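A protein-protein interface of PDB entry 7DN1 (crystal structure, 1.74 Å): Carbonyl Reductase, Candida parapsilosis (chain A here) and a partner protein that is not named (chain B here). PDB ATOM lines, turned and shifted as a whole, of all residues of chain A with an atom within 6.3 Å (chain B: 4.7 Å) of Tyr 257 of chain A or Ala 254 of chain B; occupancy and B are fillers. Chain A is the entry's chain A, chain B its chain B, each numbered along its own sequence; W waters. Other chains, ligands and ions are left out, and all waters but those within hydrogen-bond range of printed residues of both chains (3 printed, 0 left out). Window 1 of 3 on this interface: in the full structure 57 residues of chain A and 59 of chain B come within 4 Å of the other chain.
Water W3 lies within hydrogen-bond range of OH of Tyr 257 of chain A, O of Ala 262 of chain A and N of Ala 254 of chain B. Water W1 lies within hydrogen-bond range of the backbone carbonyl oxygen (O) of Ala 262 of chain A (2.7 Å), the backbone NH (N) of Gly 253 of chain B (2.9 Å) and the backbone NH (N) of Val 252 of chain B (3.5 Å). Water W2 bridges the side-chain hydroxyl (OH) of Tyr 257 of chain B (2.8 Å) and the backbone NH (N) of Gly 254 of chain A (3.0 Å).
Of the printed residues of chain B, Tyr 257 of chain A touches Gly 253 (3.7 Å), Ala 254 (3.4 Å) and Val 273 (3.8 Å). Of chain A, only Tyr 257 (3.4 Å) comes within 4 Å of Ala 254 of chain B. Printed residues of chain B within 4 Å of Thr 266 of chain A: Val 273. Of the printed residues of chain B, Gly 253 of chain A touches Tyr 257 (3.7 Å). Printed residues of chain A within 4 Å of Val 273 of chain B: Tyr 257 (3.8 Å) and Thr 266 (3.5 Å). Printed residues of chain B within 4 Å of Phe 31 of chain A: Gly 253 (3.7 Å). Arg 211 of chain A touches none of the printed residues of chain B. The nearest residue of chain A that does not touch Ala 254 of chain B is Ala 262 of chain A (4.7 Å).
Hydrophobic or aromatic side chains of chain A that line the printed part of chain B: Phe 31 and Tyr 257. Hydrophobic or aromatic side chains of chain B that line the printed part of chain A: Ala 254, Tyr 257 and Val 273. Among the printed residues, no Asp or Glu carboxylate lies within 4 Å of a Lys or Arg side-chain nitrogen of the other chain.
The backbone carbonyl oxygen (O) of Tyr 257 of chain A lies within hydrogen-bond range of the side-chain hydroxyl (OG) of Ser 263 of chain A, at 2.8 Å. The backbone carbonyl oxygen of Tyr 257 of chain A sits at hydrogen-bond distance from the side-chain hydroxyl of Ser 260 of chain A. OG1 of Thr 266 of chain A lies within hydrogen-bond range of OH of Tyr 257 of chain A. The guanidinium group (NH1) of Arg 211 of chain A is in hydrogen-bond range of the backbone carbonyl oxygen (O) of Thr 266 of chain A (3.1 Å).
Among the printed residues, pairs that only touch across the chains: Tyr 257 of chain A with Ala 254 of chain B, Gly 254 of chain A with Tyr 257 of chain B, Thr 266 of chain A with Val 273 of chain B, Tyr 257 of chain A with Gly 253 of chain B, Gly 253 of chain A with Tyr 257 of chain B, Phe 31 of chain A with Gly 253 of chain B and Tyr 257 of chain A with Val 273 of chain B.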
ATOM      1  N   PHE A  31     -33.363   6.166  19.419  1.00  0.00           N
ATOM      2  CA  PHE A  31     -32.012   6.342  19.924  1.00  0.00           C
ATOM      3  C   PHE A  31     -31.712   7.762  20.372  1.00  0.00           C
ATOM      4  O   PHE A  31     -30.613   8.014  20.875  1.00  0.00           O
ATOM      5  CB  PHE A  31     -31.003   5.900  18.854  1.00  0.00           C
ATOM      6  CG  PHE A  31     -30.936   4.422  18.697  1.00  0.00           C
ATOM      7  CD1 PHE A  31     -31.810   3.760  17.852  1.00  0.00           C
ATOM      8  CD2 PHE A  31     -30.008   3.680  19.410  1.00  0.00           C
ATOM      9  CE1 PHE A  31     -31.756   2.374  17.716  1.00  0.00           C
ATOM     10  CE2 PHE A  31     -29.953   2.293  19.287  1.00  0.00           C
ATOM     11  CZ  PHE A  31     -30.821   1.638  18.434  1.00  0.00           C
ATOM     12  N   TYR A  55     -23.205  10.635  23.931  1.00  0.00           N
ATOM     13  CA  TYR A  55     -24.475  11.042  24.516  1.00  0.00           C
ATOM     14  C   TYR A  55     -24.792  12.485  24.159  1.00  0.00           C
ATOM     15  O   TYR A  55     -25.955  12.825  23.910  1.00  0.00           O
ATOM     16  CB  TYR A  55     -24.435  10.842  26.029  1.00  0.00           C
ATOM     17  CG  TYR A  55     -24.571   9.398  26.464  1.00  0.00           C
ATOM     18  CD1 TYR A  55     -24.791   8.376  25.541  1.00  0.00           C
ATOM     19  CD2 TYR A  55     -24.523   9.063  27.807  1.00  0.00           C
ATOM     20  CE1 TYR A  55     -24.941   7.036  25.971  1.00  0.00           C
ATOM     21  CE2 TYR A  55     -24.664   7.758  28.232  1.00  0.00           C
ATOM     22  CZ  TYR A  55     -24.885   6.751  27.324  1.00  0.00           C
ATOM     23  OH  TYR A  55     -25.033   5.461  27.795  1.00  0.00           O
ATOM     24  N   ILE A 169     -26.495   2.233  33.460  1.00  0.00           N
ATOM     25  CA  ILE A 169     -25.547   1.345  32.792  1.00  0.00           C
ATOM     26  C   ILE A 169     -24.293   1.246  33.644  1.00  0.00           C
ATOM     27  O   ILE A 169     -23.714   2.272  34.021  1.00  0.00           O
ATOM     28  CB  ILE A 169     -25.195   1.852  31.378  1.00  0.00           C
ATOM     29  CG1 ILE A 169     -26.449   2.307  30.644  1.00  0.00           C
ATOM     30  CG2 ILE A 169     -24.305   0.844  30.598  1.00  0.00           C
ATOM     31  CD1 ILE A 169     -26.168   2.948  29.309  1.00  0.00           C
ATOM     32  N   ARG A 211     -34.493   0.936  34.455  1.00  0.00           N
ATOM     33  CA  ARG A 211     -33.786  -0.197  33.887  1.00  0.00           C
ATOM     34  C   ARG A 211     -32.323  -0.137  34.310  1.00  0.00           C
ATOM     35  O   ARG A 211     -31.776   0.946  34.548  1.00  0.00           O
ATOM     36  CB  ARG A 211     -33.900  -0.200  32.357  1.00  0.00           C
ATOM     37  CG  ARG A 211     -35.344  -0.365  31.869  1.00  0.00           C
ATOM     38  CD  ARG A 211     -35.407  -0.440  30.357  1.00  0.00           C
ATOM     39  NE  ARG A 211     -35.003   0.831  29.748  1.00  0.00           N
ATOM     40  CZ  ARG A 211     -33.854   1.015  29.099  1.00  0.00           C
ATOM     41  NH1 ARG A 211     -32.979   0.013  29.000  1.00  0.00           N
ATOM     42  NH2 ARG A 211     -33.564   2.211  28.568  1.00  0.00           N
ATOM     43  N   VAL A 252     -19.653   2.834  21.755  1.00  0.00           N
ATOM     44  CA  VAL A 252     -20.655   3.863  22.026  1.00  0.00           C
ATOM     45  C   VAL A 252     -22.034   3.431  21.552  1.00  0.00           C
ATOM     46  O   VAL A 252     -23.047   3.844  22.132  1.00  0.00           O
ATOM     47  CB  VAL A 252     -20.250   5.223  21.426  1.00  0.00           C
ATOM     48  CG1 VAL A 252     -18.971   5.716  22.080  1.00  0.00           C
ATOM     49  CG2 VAL A 252     -20.122   5.137  19.913  1.00  0.00           C
ATOM     50  N   GLY A 253     -22.109   2.582  20.525  1.00  0.00           N
ATOM     51  CA  GLY A 253     -23.411   2.122  20.066  1.00  0.00           C
ATOM     52  C   GLY A 253     -24.154   1.359  21.144  1.00  0.00           C
ATOM     53  O   GLY A 253     -25.360   1.554  21.349  1.00  0.00           O
ATOM     54  N   GLY A 254     -23.438   0.509  21.877  1.00  0.00           N
ATOM     55  CA  GLY A 254     -24.073  -0.238  22.952  1.00  0.00           C
ATOM     56  C   GLY A 254     -24.464   0.639  24.124  1.00  0.00           C
ATOM     57  O   GLY A 254     -25.509   0.428  24.745  1.00  0.00           O
ATOM     58  N   TYR A 255     -23.636   1.629  24.454  1.00  0.00           N
ATOM     59  CA  TYR A 255     -23.996   2.538  25.542  1.00  0.00           C
ATOM     60  C   TYR A 255     -25.200   3.399  25.172  1.00  0.00           C
ATOM     61  O   TYR A 255     -26.038   3.710  26.031  1.00  0.00           O
ATOM     62  CB  TYR A 255     -22.804   3.421  25.910  1.00  0.00           C
ATOM     63  CG  TYR A 255     -21.795   2.738  26.810  1.00  0.00           C
ATOM     64  CD1 TYR A 255     -21.903   2.811  28.200  1.00  0.00           C
ATOM     65  CD2 TYR A 255     -20.742   2.010  26.267  1.00  0.00           C
ATOM     66  CE1 TYR A 255     -20.974   2.174  29.024  1.00  0.00           C
ATOM     67  CE2 TYR A 255     -19.821   1.371  27.075  1.00  0.00           C
ATOM     68  CZ  TYR A 255     -19.935   1.461  28.449  1.00  0.00           C
ATOM     69  OH  TYR A 255     -19.006   0.819  29.241  1.00  0.00           O
ATOM     70  N   LEU A 256     -25.298   3.805  23.903  1.00  0.00           N
ATOM     71  CA  LEU A 256     -26.465   4.569  23.464  1.00  0.00           C
ATOM     72  C   LEU A 256     -27.714   3.694  23.419  1.00  0.00           C
ATOM     73  O   LEU A 256     -28.798   4.126  23.832  1.00  0.00           O
ATOM     74  CB  LEU A 256     -26.196   5.204  22.098  1.00  0.00           C
ATOM     75  CG  LEU A 256     -27.337   6.124  21.631  1.00  0.00           C
ATOM     76  CD1 LEU A 256     -27.649   7.225  22.653  1.00  0.00           C
ATOM     77  CD2 LEU A 256     -27.030   6.712  20.254  1.00  0.00           C
ATOM     78  N   TYR A 257     -27.579   2.466  22.910  1.00  0.00           N
ATOM     79  CA  TYR A 257     -28.689   1.521  22.904  1.00  0.00           C
ATOM     80  C   TYR A 257     -29.314   1.424  24.289  1.00  0.00           C
ATOM     81  O   TYR A 257     -30.526   1.603  24.446  1.00  0.00           O
ATOM     82  CB  TYR A 257     -28.206   0.142  22.420  1.00  0.00           C
ATOM     83  CG  TYR A 257     -29.233  -0.953  22.607  1.00  0.00           C
ATOM     84  CD1 TYR A 257     -30.388  -0.979  21.845  1.00  0.00           C
ATOM     85  CD2 TYR A 257     -29.049  -1.961  23.559  1.00  0.00           C
ATOM     86  CE1 TYR A 257     -31.362  -1.966  22.028  1.00  0.00           C
ATOM     87  CE2 TYR A 257     -30.020  -2.955  23.754  1.00  0.00           C
ATOM     88  CZ  TYR A 257     -31.166  -2.956  22.975  1.00  0.00           C
ATOM     89  OH  TYR A 257     -32.147  -3.927  23.141  1.00  0.00           O
ATOM     90  N   LEU A 258     -28.484   1.201  25.315  1.00  0.00           N
ATOM     91  CA  LEU A 258     -29.000   0.973  26.669  1.00  0.00           C
ATOM     92  C   LEU A 258     -29.530   2.248  27.318  1.00  0.00           C
ATOM     93  O   LEU A 258     -30.463   2.191  28.134  1.00  0.00           O
ATOM     94  CB  LEU A 258     -27.893   0.355  27.533  1.00  0.00           C
ATOM     95  CG  LEU A 258     -27.485  -1.074  27.187  1.00  0.00           C
ATOM     96  CD1 LEU A 258     -26.344  -1.523  28.083  1.00  0.00           C
ATOM     97  CD2 LEU A 258     -28.663  -2.046  27.310  1.00  0.00           C
ATOM     98  N   ALA A 259     -28.968   3.404  26.959  1.00  0.00           N
ATOM     99  CA  ALA A 259     -29.366   4.671  27.563  1.00  0.00           C
ATOM    100  C   ALA A 259     -30.717   5.157  27.050  1.00  0.00           C
ATOM    101  O   ALA A 259     -31.450   5.850  27.773  1.00  0.00           O
ATOM    102  CB  ALA A 259     -28.301   5.738  27.268  1.00  0.00           C
ATOM    103  N   SER A 260     -31.052   4.809  25.817  1.00  0.00           N
ATOM    104  CA  SER A 260     -32.138   5.433  25.081  1.00  0.00           C
ATOM    105  C   SER A 260     -33.407   4.591  25.168  1.00  0.00           C
ATOM    106  O   SER A 260     -33.445   3.535  25.806  1.00  0.00           O
ATOM    107  CB  SER A 260     -31.709   5.637  23.626  1.00  0.00           C
ATOM    108  OG  SER A 260     -31.747   4.394  22.943  1.00  0.00           O
ATOM    109  N   ASN A 261     -34.452   5.065  24.487  1.00  0.00           N
ATOM    110  CA  ASN A 261     -35.695   4.319  24.335  1.00  0.00           C
ATOM    111  C   ASN A 261     -35.605   3.207  23.304  1.00  0.00           C
ATOM    112  O   ASN A 261     -36.635   2.618  22.974  1.00  0.00           O
ATOM    113  CB  ASN A 261     -36.850   5.265  23.969  1.00  0.00           C
ATOM    114  CG  ASN A 261     -37.366   6.056  25.161  1.00  0.00           C
ATOM    115  OD1 ASN A 261     -37.016   5.781  26.310  1.00  0.00           O
ATOM    116  ND2 ASN A 261     -38.191   7.055  24.886  1.00  0.00           N
ATOM    117  N   ALA A 262     -34.410   2.891  22.788  1.00  0.00           N
ATOM    118  CA  ALA A 262     -34.269   1.728  21.926  1.00  0.00           C
ATOM    119  C   ALA A 262     -34.371   0.416  22.694  1.00  0.00           C
ATOM    120  O   ALA A 262     -34.524  -0.640  22.071  1.00  0.00           O
ATOM    121  CB  ALA A 262     -32.924   1.786  21.197  1.00  0.00           C
ATOM    122  N   SER A 263     -34.307   0.458  24.019  1.00  0.00           N
ATOM    123  CA  SER A 263     -34.104  -0.734  24.836  1.00  0.00           C
ATOM    124  C   SER A 263     -35.070  -0.777  26.012  1.00  0.00           C
ATOM    125  O   SER A 263     -34.703  -1.209  27.116  1.00  0.00           O
ATOM    126  CB  SER A 263     -32.660  -0.789  25.331  1.00  0.00           C
ATOM    127  OG  SER A 263     -32.372   0.356  26.135  1.00  0.00           O
ATOM    128  N   THR A 264     -36.324  -0.358  25.798  1.00  0.00           N
ATOM    129  CA  THR A 264     -37.252  -0.215  26.923  1.00  0.00           C
ATOM    130  C   THR A 264     -37.766  -1.548  27.473  1.00  0.00           C
ATOM    131  O   THR A 264     -38.396  -1.546  28.539  1.00  0.00           O
ATOM    132  CB  THR A 264     -38.453   0.674  26.553  1.00  0.00           C
ATOM    133  OG1 THR A 264     -39.162   0.147  25.423  1.00  0.00           O
ATOM    134  CG2 THR A 264     -38.015   2.103  26.262  1.00  0.00           C
ATOM    135  N   THR A 266     -35.362  -3.995  27.736  1.00  0.00           N
ATOM    136  CA  THR A 266     -34.074  -4.584  28.074  1.00  0.00           C
ATOM    137  C   THR A 266     -33.672  -4.171  29.481  1.00  0.00           C
ATOM    138  O   THR A 266     -33.395  -2.992  29.732  1.00  0.00           O
ATOM    139  CB  THR A 266     -33.009  -4.138  27.073  1.00  0.00           C
ATOM    140  OG1 THR A 266     -33.483  -4.367  25.737  1.00  0.00           O
ATOM    141  CG2 THR A 266     -31.702  -4.874  27.315  1.00  0.00           C
ATOM    142  N   SER A 269     -29.600  -7.088  31.541  1.00  0.00           N
ATOM    143  CA  SER A 269     -28.815  -7.812  30.554  1.00  0.00           C
ATOM    144  C   SER A 269     -27.380  -7.323  30.582  1.00  0.00           C
ATOM    145  O   SER A 269     -27.076  -6.210  31.026  1.00  0.00           O
ATOM    146  CB  SER A 269     -29.354  -7.658  29.135  1.00  0.00           C
ATOM    147  OG  SER A 269     -29.192  -6.333  28.677  1.00  0.00           O
ATOM    148  N   VAL A 271     -24.362  -6.778  27.936  1.00  0.00           N
ATOM    149  CA  VAL A 271     -24.056  -6.655  26.514  1.00  0.00           C
ATOM    150  C   VAL A 271     -22.541  -6.757  26.355  1.00  0.00           C
ATOM    151  O   VAL A 271     -21.789  -5.889  26.817  1.00  0.00           O
ATOM    152  CB  VAL A 271     -24.614  -5.346  25.937  1.00  0.00           C
ATOM    153  CG1 VAL A 271     -23.943  -4.993  24.635  1.00  0.00           C
ATOM    154  CG2 VAL A 271     -26.165  -5.436  25.806  1.00  0.00           C
ATOM    155  N   VAL B 215     -30.163 -12.390  18.951  1.00  0.00           N
ATOM    156  CA  VAL B 215     -31.099 -11.706  19.835  1.00  0.00           C
ATOM    157  C   VAL B 215     -31.952 -12.784  20.488  1.00  0.00           C
ATOM    158  O   VAL B 215     -32.461 -13.678  19.797  1.00  0.00           O
ATOM    159  CB  VAL B 215     -31.974 -10.685  19.081  1.00  0.00           C
ATOM    160  CG1 VAL B 215     -33.021 -10.080  20.025  1.00  0.00           C
ATOM    161  CG2 VAL B 215     -31.127  -9.548  18.490  1.00  0.00           C
ATOM    162  N   LEU B 251     -37.934  -4.587  20.232  1.00  0.00           N
ATOM    163  CA  LEU B 251     -36.860  -5.444  19.753  1.00  0.00           C
ATOM    164  C   LEU B 251     -36.043  -4.795  18.655  1.00  0.00           C
ATOM    165  O   LEU B 251     -34.872  -5.162  18.478  1.00  0.00           O
ATOM    166  CB  LEU B 251     -37.416  -6.764  19.209  1.00  0.00           C
ATOM    167  CG  LEU B 251     -38.171  -7.703  20.150  1.00  0.00           C
ATOM    168  CD1 LEU B 251     -38.725  -8.863  19.353  1.00  0.00           C
ATOM    169  CD2 LEU B 251     -37.232  -8.203  21.217  1.00  0.00           C
ATOM    170  N   VAL B 252     -36.626  -3.842  17.922  1.00  0.00           N
ATOM    171  CA  VAL B 252     -35.992  -3.436  16.674  1.00  0.00           C
ATOM    172  C   VAL B 252     -34.685  -2.700  16.915  1.00  0.00           C
ATOM    173  O   VAL B 252     -33.793  -2.732  16.061  1.00  0.00           O
ATOM    174  CB  VAL B 252     -36.949  -2.595  15.815  1.00  0.00           C
ATOM    175  CG1 VAL B 252     -38.096  -3.447  15.334  1.00  0.00           C
ATOM    176  CG2 VAL B 252     -37.428  -1.383  16.604  1.00  0.00           C
ATOM    177  N   GLY B 253     -34.532  -2.030  18.056  1.00  0.00           N
ATOM    178  CA  GLY B 253     -33.265  -1.362  18.326  1.00  0.00           C
ATOM    179  C   GLY B 253     -32.115  -2.336  18.465  1.00  0.00           C
ATOM    180  O   GLY B 253     -30.998  -2.064  18.018  1.00  0.00           O
ATOM    181  N   ALA B 254     -32.365  -3.495  19.081  1.00  0.00           N
ATOM    182  CA  ALA B 254     -31.296  -4.487  19.200  1.00  0.00           C
ATOM    183  C   ALA B 254     -30.929  -5.073  17.844  1.00  0.00           C
ATOM    184  O   ALA B 254     -29.747  -5.322  17.566  1.00  0.00           O
ATOM    185  CB  ALA B 254     -31.710  -5.596  20.165  1.00  0.00           C
ATOM    186  N   TYR B 255     -31.928  -5.301  16.988  1.00  0.00           N
ATOM    187  CA  TYR B 255     -31.643  -5.831  15.663  1.00  0.00           C
ATOM    188  C   TYR B 255     -30.895  -4.808  14.819  1.00  0.00           C
ATOM    189  O   TYR B 255     -30.027  -5.175  14.019  1.00  0.00           O
ATOM    190  CB  TYR B 255     -32.929  -6.270  14.959  1.00  0.00           C
ATOM    191  CG  TYR B 255     -33.464  -7.615  15.416  1.00  0.00           C
ATOM    192  CD1 TYR B 255     -33.036  -8.802  14.812  1.00  0.00           C
ATOM    193  CD2 TYR B 255     -34.389  -7.699  16.447  1.00  0.00           C
ATOM    194  CE1 TYR B 255     -33.518 -10.041  15.235  1.00  0.00           C
ATOM    195  CE2 TYR B 255     -34.882  -8.931  16.878  1.00  0.00           C
ATOM    196  CZ  TYR B 255     -34.448 -10.089  16.270  1.00  0.00           C
ATOM    197  OH  TYR B 255     -34.957 -11.294  16.697  1.00  0.00           O
ATOM    198  N   LEU B 256     -31.214  -3.521  14.981  1.00  0.00           N
ATOM    199  CA  LEU B 256     -30.480  -2.505  14.228  1.00  0.00           C
ATOM    200  C   LEU B 256     -29.073  -2.327  14.775  1.00  0.00           C
ATOM    201  O   LEU B 256     -28.121  -2.122  14.008  1.00  0.00           O
ATOM    202  CB  LEU B 256     -31.237  -1.174  14.246  1.00  0.00           C
ATOM    203  CG  LEU B 256     -30.558  -0.068  13.422  1.00  0.00           C
ATOM    204  CD1 LEU B 256     -30.471  -0.439  11.952  1.00  0.00           C
ATOM    205  CD2 LEU B 256     -31.320   1.259  13.620  1.00  0.00           C
ATOM    206  N   TYR B 257     -28.925  -2.393  16.097  1.00  0.00           N
ATOM    207  CA  TYR B 257     -27.603  -2.350  16.711  1.00  0.00           C
ATOM    208  C   TYR B 257     -26.677  -3.384  16.078  1.00  0.00           C
ATOM    209  O   TYR B 257     -25.572  -3.058  15.620  1.00  0.00           O
ATOM    210  CB  TYR B 257     -27.726  -2.573  18.228  1.00  0.00           C
ATOM    211  CG  TYR B 257     -26.376  -2.788  18.853  1.00  0.00           C
ATOM    212  CD1 TYR B 257     -25.470  -1.737  18.945  1.00  0.00           C
ATOM    213  CD2 TYR B 257     -25.986  -4.037  19.316  1.00  0.00           C
ATOM    214  CE1 TYR B 257     -24.205  -1.916  19.488  1.00  0.00           C
ATOM    215  CE2 TYR B 257     -24.707  -4.228  19.861  1.00  0.00           C
ATOM    216  CZ  TYR B 257     -23.837  -3.160  19.951  1.00  0.00           C
ATOM    217  OH  TYR B 257     -22.572  -3.344  20.494  1.00  0.00           O
ATOM    218  N   LEU B 258     -27.124  -4.641  16.018  1.00  0.00           N
ATOM    219  CA  LEU B 258     -26.242  -5.711  15.548  1.00  0.00           C
ATOM    220  C   LEU B 258     -26.057  -5.684  14.035  1.00  0.00           C
ATOM    221  O   LEU B 258     -25.020  -6.138  13.526  1.00  0.00           O
ATOM    222  CB  LEU B 258     -26.795  -7.065  15.966  1.00  0.00           C
ATOM    223  CG  LEU B 258     -26.859  -7.326  17.472  1.00  0.00           C
ATOM    224  CD1 LEU B 258     -27.646  -8.585  17.713  1.00  0.00           C
ATOM    225  CD2 LEU B 258     -25.441  -7.425  18.053  1.00  0.00           C
ATOM    226  N   LEU B 271     -27.797 -10.954  22.815  1.00  0.00           N
ATOM    227  CA  LEU B 271     -28.484  -9.802  23.394  1.00  0.00           C
ATOM    228  C   LEU B 271     -29.852 -10.252  23.897  1.00  0.00           C
ATOM    229  O   LEU B 271     -30.745 -10.552  23.094  1.00  0.00           O
ATOM    230  CB  LEU B 271     -28.656  -8.679  22.375  1.00  0.00           C
ATOM    231  CG  LEU B 271     -27.482  -7.749  22.113  1.00  0.00           C
ATOM    232  CD1 LEU B 271     -26.292  -8.506  21.631  1.00  0.00           C
ATOM    233  CD2 LEU B 271     -27.946  -6.708  21.097  1.00  0.00           C
ATOM    234  N   VAL B 273     -33.395  -9.622  25.376  1.00  0.00           N
ATOM    235  CA  VAL B 273     -34.402  -8.573  25.451  1.00  0.00           C
ATOM    236  C   VAL B 273     -35.661  -9.195  26.028  1.00  0.00           C
ATOM    237  O   VAL B 273     -36.544  -9.615  25.274  1.00  0.00           O
ATOM    238  CB  VAL B 273     -34.660  -7.949  24.065  1.00  0.00           C
ATOM    239  CG1 VAL B 273     -35.612  -6.735  24.207  1.00  0.00           C
ATOM    240  CG2 VAL B 273     -33.369  -7.517  23.438  1.00  0.00           C
HETATM  241  O   HOH W   1     -36.381  -1.152  20.124  1.00  0.00           O
HETATM  242  O   HOH W   2     -21.179  -0.937  20.449  1.00  0.00           O
HETATM  243  O   HOH W   3     -34.201  -3.453  21.550  1.00  0.00           O
